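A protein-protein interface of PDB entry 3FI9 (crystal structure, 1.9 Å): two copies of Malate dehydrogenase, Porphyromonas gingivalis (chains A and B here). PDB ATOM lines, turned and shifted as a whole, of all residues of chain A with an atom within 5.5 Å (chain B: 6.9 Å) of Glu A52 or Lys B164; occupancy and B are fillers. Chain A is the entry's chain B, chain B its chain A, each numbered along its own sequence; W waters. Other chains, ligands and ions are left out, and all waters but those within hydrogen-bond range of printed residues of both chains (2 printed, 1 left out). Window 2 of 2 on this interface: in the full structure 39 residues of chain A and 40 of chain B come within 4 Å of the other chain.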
ATOM      1  N   LEU A  47     -27.165 -31.486  20.298  1.00  0.00           N
ATOM      2  CA  LEU A  47     -27.598 -31.481  18.920  1.00  0.00           C
ATOM      3  C   LEU A  47     -27.774 -30.048  18.398  1.00  0.00           C
ATOM      4  O   LEU A  47     -27.362 -29.719  17.283  1.00  0.00           O
ATOM      5  CB  LEU A  47     -28.917 -32.247  18.792  1.00  0.00           C
ATOM      6  CG  LEU A  47     -29.572 -32.400  17.418  1.00  0.00           C
ATOM      7  CD1 LEU A  47     -28.632 -33.161  16.422  1.00  0.00           C
ATOM      8  CD2 LEU A  47     -30.864 -33.143  17.608  1.00  0.00           C
ATOM      9  N   GLU A  48     -28.419 -29.202  19.199  1.00  0.00           N
ATOM     10  CA  GLU A  48     -28.637 -27.838  18.763  1.00  0.00           C
ATOM     11  C   GLU A  48     -27.316 -27.126  18.484  1.00  0.00           C
ATOM     12  O   GLU A  48     -27.223 -26.320  17.555  1.00  0.00           O
ATOM     13  CB  GLU A  48     -29.448 -27.068  19.803  1.00  0.00           C
ATOM     14  CG  GLU A  48     -29.715 -25.638  19.401  1.00  0.00           C
ATOM     15  CD  GLU A  48     -30.495 -24.884  20.485  1.00  0.00           C
ATOM     16  OE1 GLU A  48     -30.943 -25.510  21.456  1.00  0.00           O
ATOM     17  OE2 GLU A  48     -30.680 -23.677  20.341  1.00  0.00           O
ATOM     18  N   GLY A  49     -26.302 -27.399  19.289  1.00  0.00           N
ATOM     19  CA  GLY A  49     -25.007 -26.751  19.114  1.00  0.00           C
ATOM     20  C   GLY A  49     -24.363 -27.179  17.806  1.00  0.00           C
ATOM     21  O   GLY A  49     -23.734 -26.371  17.125  1.00  0.00           O
ATOM     22  N   VAL A  50     -24.549 -28.446  17.449  1.00  0.00           N
ATOM     23  CA  VAL A  50     -24.043 -28.964  16.153  1.00  0.00           C
ATOM     24  C   VAL A  50     -24.805 -28.281  15.029  1.00  0.00           C
ATOM     25  O   VAL A  50     -24.176 -27.779  14.121  1.00  0.00           O
ATOM     26  CB  VAL A  50     -24.154 -30.489  16.047  1.00  0.00           C
ATOM     27  CG1 VAL A  50     -23.808 -30.994  14.597  1.00  0.00           C
ATOM     28  CG2 VAL A  50     -23.242 -31.160  17.106  1.00  0.00           C
ATOM     29  N   ALA A  51     -26.147 -28.212  15.113  1.00  0.00           N
ATOM     30  CA  ALA A  51     -26.947 -27.586  14.033  1.00  0.00           C
ATOM     31  C   ALA A  51     -26.554 -26.111  13.882  1.00  0.00           C
ATOM     32  O   ALA A  51     -26.351 -25.619  12.754  1.00  0.00           O
ATOM     33  CB  ALA A  51     -28.467 -27.756  14.282  1.00  0.00           C
ATOM     34  N   GLU A  52     -26.306 -25.432  15.009  1.00  0.00           N
ATOM     35  CA  GLU A  52     -25.855 -24.030  14.952  1.00  0.00           C
ATOM     36  C   GLU A  52     -24.517 -23.887  14.207  1.00  0.00           C
ATOM     37  O   GLU A  52     -24.383 -23.041  13.293  1.00  0.00           O
ATOM     38  CB  GLU A  52     -25.769 -23.390  16.346  1.00  0.00           C
ATOM     39  CG  GLU A  52     -27.142 -23.222  17.072  1.00  0.00           C
ATOM     40  CD  GLU A  52     -28.159 -22.270  16.369  1.00  0.00           C
ATOM     41  OE1 GLU A  52     -28.195 -22.156  15.123  1.00  0.00           O
ATOM     42  OE2 GLU A  52     -28.966 -21.616  17.076  1.00  0.00           O
ATOM     43  N   GLU A  53     -23.540 -24.710  14.562  1.00  0.00           N
ATOM     44  CA  GLU A  53     -22.270 -24.703  13.818  1.00  0.00           C
ATOM     45  C   GLU A  53     -22.466 -24.927  12.340  1.00  0.00           C
ATOM     46  O   GLU A  53     -21.826 -24.252  11.520  1.00  0.00           O
ATOM     47  CB  GLU A  53     -21.329 -25.751  14.388  1.00  0.00           C
ATOM     48  CG  GLU A  53     -20.599 -25.300  15.696  1.00  0.00           C
ATOM     49  CD  GLU A  53     -19.060 -25.264  15.463  1.00  0.00           C
ATOM     50  OE1 GLU A  53     -18.327 -26.040  16.103  1.00  0.00           O
ATOM     51  OE2 GLU A  53     -18.589 -24.461  14.625  1.00  0.00           O
ATOM     52  N   ILE A  54     -23.301 -25.910  11.973  1.00  0.00           N
ATOM     53  CA  ILE A  54     -23.485 -26.178  10.560  1.00  0.00           C
ATOM     54  C   ILE A  54     -24.125 -24.946   9.884  1.00  0.00           C
ATOM     55  O   ILE A  54     -23.729 -24.543   8.799  1.00  0.00           O
ATOM     56  CB  ILE A  54     -24.351 -27.440  10.298  1.00  0.00           C
ATOM     57  CG1 ILE A  54     -23.691 -28.662  10.933  1.00  0.00           C
ATOM     58  CG2 ILE A  54     -24.716 -27.597   8.760  1.00  0.00           C
ATOM     59  CD1 ILE A  54     -22.295 -29.011  10.367  1.00  0.00           C
ATOM     60  N   ARG A  55     -25.110 -24.360  10.525  1.00  0.00           N
ATOM     61  CA  ARG A  55     -25.781 -23.167   9.931  1.00  0.00           C
ATOM     62  C   ARG A  55     -24.775 -22.015   9.720  1.00  0.00           C
ATOM     63  O   ARG A  55     -24.869 -21.239   8.759  1.00  0.00           O
ATOM     64  CB  ARG A  55     -26.871 -22.717  10.888  1.00  0.00           C
ATOM     65  CG  ARG A  55     -28.121 -23.591  10.844  1.00  0.00           C
ATOM     66  CD  ARG A  55     -28.936 -23.274  12.119  1.00  0.00           C
ATOM     67  NE  ARG A  55     -30.279 -23.821  12.032  1.00  0.00           N
ATOM     68  CZ  ARG A  55     -31.126 -23.920  13.062  1.00  0.00           C
ATOM     69  NH1 ARG A  55     -32.342 -24.422  12.872  1.00  0.00           N
ATOM     70  NH2 ARG A  55     -30.757 -23.539  14.286  1.00  0.00           N
ATOM     71  N   HIS A  56     -23.848 -21.863  10.668  1.00  0.00           N
ATOM     72  CA  HIS A  56     -22.843 -20.828  10.575  1.00  0.00           C
ATOM     73  C   HIS A  56     -21.752 -21.069   9.532  1.00  0.00           C
ATOM     74  O   HIS A  56     -20.959 -20.160   9.248  1.00  0.00           O
ATOM     75  CB  HIS A  56     -22.214 -20.541  11.957  1.00  0.00           C
ATOM     76  CG  HIS A  56     -23.232 -20.263  13.043  1.00  0.00           C
ATOM     77  ND1 HIS A  56     -22.913 -20.298  14.370  1.00  0.00           N
ATOM     78  CD2 HIS A  56     -24.560 -19.975  12.986  1.00  0.00           C
ATOM     79  CE1 HIS A  56     -23.989 -20.050  15.101  1.00  0.00           C
ATOM     80  NE2 HIS A  56     -25.000 -19.836  14.283  1.00  0.00           N
ATOM     81  N   CYS A  57     -21.698 -22.253   8.924  1.00  0.00           N
ATOM     82  CA  CYS A  57     -20.820 -22.435   7.741  1.00  0.00           C
ATOM     83  C   CYS A  57     -21.359 -21.746   6.494  1.00  0.00           C
ATOM     84  O   CYS A  57     -20.592 -21.423   5.569  1.00  0.00           O
ATOM     85  CB  CYS A  57     -20.631 -23.915   7.437  1.00  0.00           C
ATOM     86  SG  CYS A  57     -19.777 -24.809   8.739  1.00  0.00           S
ATOM     87  N   ARG B 157     -23.837 -15.850  11.090  1.00  0.00           N
ATOM     88  CA  ARG B 157     -24.680 -15.998  12.269  1.00  0.00           C
ATOM     89  C   ARG B 157     -25.878 -15.035  12.131  1.00  0.00           C
ATOM     90  O   ARG B 157     -27.017 -15.395  12.399  1.00  0.00           O
ATOM     91  CB  ARG B 157     -23.879 -15.722  13.520  1.00  0.00           C
ATOM     92  CG  ARG B 157     -22.913 -16.864  13.829  1.00  0.00           C
ATOM     93  CD  ARG B 157     -22.020 -16.524  15.075  1.00  0.00           C
ATOM     94  NE  ARG B 157     -21.104 -17.631  15.325  1.00  0.00           N
ATOM     95  CZ  ARG B 157     -20.021 -17.547  16.102  1.00  0.00           C
ATOM     96  NH1 ARG B 157     -19.716 -16.415  16.708  1.00  0.00           N
ATOM     97  NH2 ARG B 157     -19.239 -18.602  16.280  1.00  0.00           N
ATOM     98  N   LEU B 158     -25.633 -13.829  11.658  1.00  0.00           N
ATOM     99  CA  LEU B 158     -26.779 -12.936  11.418  1.00  0.00           C
ATOM    100  C   LEU B 158     -27.760 -13.549  10.411  1.00  0.00           C
ATOM    101  O   LEU B 158     -28.979 -13.485  10.591  1.00  0.00           O
ATOM    102  CB  LEU B 158     -26.321 -11.544  10.996  1.00  0.00           C
ATOM    103  CG  LEU B 158     -27.411 -10.508  10.673  1.00  0.00           C
ATOM    104  CD1 LEU B 158     -28.207 -10.169  11.897  1.00  0.00           C
ATOM    105  CD2 LEU B 158     -26.750  -9.209  10.158  1.00  0.00           C
ATOM    106  N   GLN B 159     -27.227 -14.137   9.350  1.00  0.00           N
ATOM    107  CA  GLN B 159     -28.072 -14.814   8.366  1.00  0.00           C
ATOM    108  C   GLN B 159     -28.890 -15.919   9.008  1.00  0.00           C
ATOM    109  O   GLN B 159     -30.111 -16.022   8.795  1.00  0.00           O
ATOM    110  CB  GLN B 159     -27.239 -15.369   7.197  1.00  0.00           C
ATOM    111  CG  GLN B 159     -28.103 -15.988   6.066  1.00  0.00           C
ATOM    112  CD  GLN B 159     -27.277 -16.770   5.059  1.00  0.00           C
ATOM    113  OE1 GLN B 159     -26.472 -17.624   5.453  1.00  0.00           O
ATOM    114  NE2 GLN B 159     -27.473 -16.500   3.762  1.00  0.00           N
ATOM    115  N   SER B 160     -28.228 -16.755   9.791  1.00  0.00           N
ATOM    116  CA  SER B 160     -28.922 -17.844  10.459  1.00  0.00           C
ATOM    117  C   SER B 160     -30.029 -17.361  11.413  1.00  0.00           C
ATOM    118  O   SER B 160     -31.169 -17.841  11.378  1.00  0.00           O
ATOM    119  CB  SER B 160     -27.909 -18.688  11.227  1.00  0.00           C
ATOM    120  OG  SER B 160     -28.568 -19.706  11.969  1.00  0.00           O
ATOM    121  N   GLU B 161     -29.690 -16.401  12.254  1.00  0.00           N
ATOM    122  CA  GLU B 161     -30.634 -15.883  13.232  1.00  0.00           C
ATOM    123  C   GLU B 161     -31.840 -15.238  12.555  1.00  0.00           C
ATOM    124  O   GLU B 161     -32.956 -15.468  12.991  1.00  0.00           O
ATOM    125  CB  GLU B 161     -29.950 -14.940  14.241  1.00  0.00           C
ATOM    126  CG  GLU B 161     -28.859 -15.598  15.150  1.00  0.00           C
ATOM    127  CD  GLU B 161     -29.396 -16.660  16.097  1.00  0.00           C
ATOM    128  OE1 GLU B 161     -30.532 -16.537  16.610  1.00  0.00           O
ATOM    129  OE2 GLU B 161     -28.664 -17.629  16.353  1.00  0.00           O
ATOM    130  N   LEU B 162     -31.634 -14.495  11.454  1.00  0.00           N
ATOM    131  CA  LEU B 162     -32.750 -13.966  10.634  1.00  0.00           C
ATOM    132  C   LEU B 162     -33.610 -15.058  10.000  1.00  0.00           C
ATOM    133  O   LEU B 162     -34.859 -14.978  10.028  1.00  0.00           O
ATOM    134  CB  LEU B 162     -32.246 -13.011   9.556  1.00  0.00           C
ATOM    135  CG  LEU B 162     -31.895 -11.594  10.074  1.00  0.00           C
ATOM    136  CD1 LEU B 162     -31.000 -10.915   9.066  1.00  0.00           C
ATOM    137  CD2 LEU B 162     -33.182 -10.758  10.319  1.00  0.00           C
ATOM    138  N   ALA B 163     -32.970 -16.087   9.444  1.00  0.00           N
ATOM    139  CA  ALA B 163     -33.739 -17.182   8.862  1.00  0.00           C
ATOM    140  C   ALA B 163     -34.574 -17.931   9.920  1.00  0.00           C
ATOM    141  O   ALA B 163     -35.738 -18.252   9.674  1.00  0.00           O
ATOM    142  CB  ALA B 163     -32.817 -18.158   8.052  1.00  0.00           C
ATOM    143  N   LYS B 164     -34.015 -18.130  11.105  1.00  0.00           N
ATOM    144  CA  LYS B 164     -34.773 -18.733  12.208  1.00  0.00           C
ATOM    145  C   LYS B 164     -35.988 -17.895  12.637  1.00  0.00           C
ATOM    146  O   LYS B 164     -37.080 -18.442  12.860  1.00  0.00           O
ATOM    147  CB  LYS B 164     -33.857 -18.972  13.414  1.00  0.00           C
ATOM    148  CG  LYS B 164     -32.812 -20.092  13.188  1.00  0.00           C
ATOM    149  CD  LYS B 164     -31.599 -19.957  14.118  1.00  0.00           C
ATOM    150  CE  LYS B 164     -31.991 -19.879  15.581  1.00  0.00           C
ATOM    151  NZ  LYS B 164     -30.786 -19.934  16.471  1.00  0.00           N
ATOM    152  N   HIS B 165     -35.778 -16.585  12.803  1.00  0.00           N
ATOM    153  CA  HIS B 165     -36.862 -15.655  13.149  1.00  0.00           C
ATOM    154  C   HIS B 165     -38.021 -15.751  12.161  1.00  0.00           C
ATOM    155  O   HIS B 165     -39.188 -15.825  12.552  1.00  0.00           O
ATOM    156  CB  HIS B 165     -36.376 -14.185  13.209  1.00  0.00           C
ATOM    157  CG  HIS B 165     -37.478 -13.222  13.516  1.00  0.00           C
ATOM    158  ND1 HIS B 165     -37.951 -13.020  14.799  1.00  0.00           N
ATOM    159  CD2 HIS B 165     -38.270 -12.482  12.701  1.00  0.00           C
ATOM    160  CE1 HIS B 165     -38.946 -12.150  14.765  1.00  0.00           C
ATOM    161  NE2 HIS B 165     -39.163 -11.815  13.504  1.00  0.00           N
ATOM    162  N   PHE B 166     -37.696 -15.752  10.880  1.00  0.00           N
ATOM    163  CA  PHE B 166     -38.723 -15.706   9.823  1.00  0.00           C
ATOM    164  C   PHE B 166     -39.208 -17.097   9.453  1.00  0.00           C
ATOM    165  O   PHE B 166     -40.171 -17.256   8.723  1.00  0.00           O
ATOM    166  CB  PHE B 166     -38.199 -14.955   8.601  1.00  0.00           C
ATOM    167  CG  PHE B 166     -38.172 -13.448   8.789  1.00  0.00           C
ATOM    168  CD1 PHE B 166     -39.356 -12.705   8.739  1.00  0.00           C
ATOM    169  CD2 PHE B 166     -36.984 -12.789   9.053  1.00  0.00           C
ATOM    170  CE1 PHE B 166     -39.350 -11.309   8.911  1.00  0.00           C
ATOM    171  CE2 PHE B 166     -36.958 -11.384   9.224  1.00  0.00           C
ATOM    172  CZ  PHE B 166     -38.138 -10.655   9.166  1.00  0.00           C
ATOM    173  N   GLY B 167     -38.557 -18.109  10.018  1.00  0.00           N
ATOM    174  CA  GLY B 167     -38.946 -19.481   9.759  1.00  0.00           C
ATOM    175  C   GLY B 167     -38.758 -19.852   8.304  1.00  0.00           C
ATOM    176  O   GLY B 167     -39.593 -20.555   7.738  1.00  0.00           O
ATOM    177  N   ILE B 168     -37.691 -19.364   7.665  1.00  0.00           N
ATOM    178  CA  ILE B 168     -37.444 -19.701   6.263  1.00  0.00           C
ATOM    179  C   ILE B 168     -36.078 -20.340   6.030  1.00  0.00           C
ATOM    180  O   ILE B 168     -35.169 -20.266   6.860  1.00  0.00           O
ATOM    181  CB  ILE B 168     -37.525 -18.494   5.288  1.00  0.00           C
ATOM    182  CG1 ILE B 168     -36.475 -17.433   5.664  1.00  0.00           C
ATOM    183  CG2 ILE B 168     -38.953 -17.896   5.281  1.00  0.00           C
ATOM    184  CD1 ILE B 168     -36.568 -16.218   4.788  1.00  0.00           C
ATOM    185  N   GLN B 170     -32.384 -20.813   5.235  1.00  0.00           N
ATOM    186  CA  GLN B 170     -31.356 -19.820   5.503  1.00  0.00           C
ATOM    187  C   GLN B 170     -30.844 -19.031   4.301  1.00  0.00           C
ATOM    188  O   GLN B 170     -30.633 -17.823   4.404  1.00  0.00           O
ATOM    189  CB  GLN B 170     -30.188 -20.461   6.247  1.00  0.00           C
ATOM    190  CG  GLN B 170     -29.131 -19.472   6.656  1.00  0.00           C
ATOM    191  CD  GLN B 170     -28.102 -20.148   7.563  1.00  0.00           C
ATOM    192  OE1 GLN B 170     -28.412 -21.116   8.260  1.00  0.00           O
ATOM    193  NE2 GLN B 170     -26.869 -19.665   7.510  1.00  0.00           N
ATOM    194  N   VAL B 173     -32.122 -15.557   3.052  1.00  0.00           N
ATOM    195  CA  VAL B 173     -31.735 -14.266   3.649  1.00  0.00           C
ATOM    196  C   VAL B 173     -30.403 -13.891   2.953  1.00  0.00           C
ATOM    197  O   VAL B 173     -29.389 -14.541   3.161  1.00  0.00           O
ATOM    198  CB  VAL B 173     -31.555 -14.377   5.183  1.00  0.00           C
ATOM    199  CG1 VAL B 173     -31.165 -13.021   5.786  1.00  0.00           C
ATOM    200  CG2 VAL B 173     -32.818 -14.869   5.843  1.00  0.00           C
ATOM    201  N   LEU B 217     -32.281 -10.368  18.612  1.00  0.00           N
ATOM    202  CA  LEU B 217     -31.665 -11.129  17.524  1.00  0.00           C
ATOM    203  C   LEU B 217     -30.193 -10.710  17.345  1.00  0.00           C
ATOM    204  O   LEU B 217     -29.293 -11.562  17.265  1.00  0.00           O
ATOM    205  CB  LEU B 217     -32.482 -10.957  16.239  1.00  0.00           C
ATOM    206  CG  LEU B 217     -32.188 -11.827  15.016  1.00  0.00           C
ATOM    207  CD1 LEU B 217     -33.375 -11.961  14.093  1.00  0.00           C
ATOM    208  CD2 LEU B 217     -31.011 -11.299  14.246  1.00  0.00           C
ATOM    209  N   ARG B 220     -28.123 -12.241  19.956  1.00  0.00           N
ATOM    210  CA  ARG B 220     -27.804 -13.675  19.781  1.00  0.00           C
ATOM    211  C   ARG B 220     -26.623 -13.844  18.822  1.00  0.00           C
ATOM    212  O   ARG B 220     -25.899 -14.831  18.907  1.00  0.00           O
ATOM    213  CB  ARG B 220     -28.989 -14.496  19.247  1.00  0.00           C
ATOM    214  CG  ARG B 220     -30.172 -14.590  20.237  1.00  0.00           C
ATOM    215  CD  ARG B 220     -31.195 -15.620  19.841  1.00  0.00           C
ATOM    216  NE  ARG B 220     -31.976 -15.216  18.677  1.00  0.00           N
ATOM    217  CZ  ARG B 220     -33.045 -14.425  18.722  1.00  0.00           C
ATOM    218  NH1 ARG B 220     -33.453 -13.941  19.883  1.00  0.00           N
ATOM    219  NH2 ARG B 220     -33.698 -14.102  17.607  1.00  0.00           N
ATOM    220  N   GLY B 224     -22.986 -15.314  19.925  1.00  0.00           N
ATOM    221  CA  GLY B 224     -23.041 -16.581  19.181  1.00  0.00           C
ATOM    222  C   GLY B 224     -21.977 -17.593  19.597  1.00  0.00           C
ATOM    223  O   GLY B 224     -22.249 -18.791  19.633  1.00  0.00           O
ATOM    224  N   ASN B 227     -22.795 -19.047  23.003  1.00  0.00           N
ATOM    225  CA  ASN B 227     -23.911 -19.978  22.844  1.00  0.00           C
ATOM    226  C   ASN B 227     -23.391 -21.350  22.348  1.00  0.00           C
ATOM    227  O   ASN B 227     -23.796 -22.388  22.875  1.00  0.00           O
ATOM    228  CB  ASN B 227     -24.945 -19.371  21.869  1.00  0.00           C
ATOM    229  CG  ASN B 227     -26.200 -20.261  21.679  1.00  0.00           C
ATOM    230  OD1 ASN B 227     -26.939 -20.531  22.622  1.00  0.00           O
ATOM    231  ND2 ASN B 227     -26.445 -20.678  20.457  1.00  0.00           N
ATOM    232  N   ILE B 228     -22.503 -21.377  21.339  1.00  0.00           N
ATOM    233  CA  ILE B 228     -21.944 -22.681  20.912  1.00  0.00           C
ATOM    234  C   ILE B 228     -21.285 -23.374  22.127  1.00  0.00           C
ATOM    235  O   ILE B 228     -21.474 -24.556  22.364  1.00  0.00           O
ATOM    236  CB  ILE B 228     -20.901 -22.560  19.752  1.00  0.00           C
ATOM    237  CG1 ILE B 228     -21.556 -21.945  18.504  1.00  0.00           C
ATOM    238  CG2 ILE B 228     -20.205 -23.940  19.431  1.00  0.00           C
ATOM    239  CD1 ILE B 228     -22.847 -22.593  18.153  1.00  0.00           C
ATOM    240  N   LEU B 231     -23.776 -24.896  24.328  1.00  0.00           N
ATOM    241  CA  LEU B 231     -24.518 -26.025  23.757  1.00  0.00           C
ATOM    242  C   LEU B 231     -23.622 -27.234  23.447  1.00  0.00           C
ATOM    243  O   LEU B 231     -24.032 -28.369  23.687  1.00  0.00           O
ATOM    244  CB  LEU B 231     -25.293 -25.596  22.533  1.00  0.00           C
ATOM    245  CG  LEU B 231     -26.263 -24.426  22.632  1.00  0.00           C
ATOM    246  CD1 LEU B 231     -26.658 -24.045  21.213  1.00  0.00           C
ATOM    247  CD2 LEU B 231     -27.504 -24.781  23.437  1.00  0.00           C
ATOM    248  N   SER B 239     -17.322 -24.401  12.185  1.00  0.00           N
ATOM    249  CA  SER B 239     -17.576 -23.232  11.323  1.00  0.00           C
ATOM    250  C   SER B 239     -16.345 -22.333  11.061  1.00  0.00           C
ATOM    251  O   SER B 239     -16.115 -21.950   9.922  1.00  0.00           O
ATOM    252  CB  SER B 239     -18.844 -22.433  11.714  1.00  0.00           C
ATOM    253  OG  SER B 239     -18.815 -22.045  13.113  1.00  0.00           O
HETATM  254  O   HOH W   1     -20.374 -21.089  15.048  1.00  0.00           O
HETATM  255  O   HOH W   2     -27.785 -19.269  14.483  1.00  0.00           O
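Of the 21 printed residues of chain B, 7 touch a printed residue of chain A.
Hydrophobic or aromatic side chains of chain A that line the printed part of chain B: His A56.
OE2 of Glu A52 lies within salt-bridge range of NZ of Lys B164, 2.6 Å away.
The backbone NH (N) of Ser B239 is in hydrogen-bond range of the side-chain carboxylate (OE2) of Glu A53 (2.7 Å).
The side-chain amide nitrogen (NE2) of Gln B170 is in hydrogen-bond range of the backbone carbonyl oxygen (O) of Arg A55 (2.8 Å).
A ring nitrogen (ND1) of His A56 lies within hydrogen-bond range of the guanidinium group of Arg B157 (3.4 Å).
No position is printed for both chains.
Of the 13 pairs that touch across the chains among the printed residues, none has its exchanged pair printed and touching as well.
CD1 of Leu B231 touches CG of Glu A48, at 3.9 Å.
Gly A49 touches Leu B231 (CA to CB, 3.6 Å).
CD1 of Ile B228 touches CB of Glu A52, at 3.5 Å.
Glu A53 touches Ile B228.
Ser B160 touches Arg A55.
Arg A55 touches Lys B164 (NH2 to CD, 3.7 Å).
CB of Ser B160 touches CD2 of His A56, 3.996 Å away.
His A56 touches Ser B239 (CB to CB, 3.9 Å).
Cys A57 touches Ser B239.
The side-chain sulfur of Cys A57 is in hydrogen-bond range of the backbone carbonyl oxygen of Glu A53 (3.5 Å).
The side-chain amide oxygen of Gln B159 sits at hydrogen-bond distance from the side-chain amide nitrogen of Gln B170.
The side-chain amino group of Lys B164 is in salt-bridge range of the side-chain carboxylate of Glu B161, at 3.1 Å.
O of Glu A52 sits close to ND1 of His A56.
The side-chain carboxylate (OE1) of Glu A52 lies within salt-bridge range of the guanidinium group (NH2) of Arg A55, 3.0 Å away.
Water W2 lies within hydrogen-bond range of the side-chain carboxylate (OE2) of Glu B161 (2.6 Å), the side-chain hydroxyl (OG) of Ser B160 (2.7 Å), a ring nitrogen (NE2) of His A56 (2.8 Å) and the side-chain carboxylate (OE1) of Glu A52 (3.0 Å).
Water W1 lies within hydrogen-bond range of OG of Ser B239, ND1 of His A56 and NH2 of Arg B157.
Of the printed residues of chain B, Glu A52 touches Lys B164 and Ile B228.
Of the printed residues of chain B, Glu A53 touches Ile B228 and Ser B239.
Of the printed residues of chain B, His A56 touches Arg B157 (3.4 Å), Ser B160 (3.996 Å) and Ser B239 (3.9 Å).
Val B173 touches none of the printed residues of chain A.
The nearest residue of chain A that does not touch Lys B164 is Glu A48 (5.4 Å).
The nearest printed residue of chain A that does not touch Ser B239 is Ile A54 (5.7 Å).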
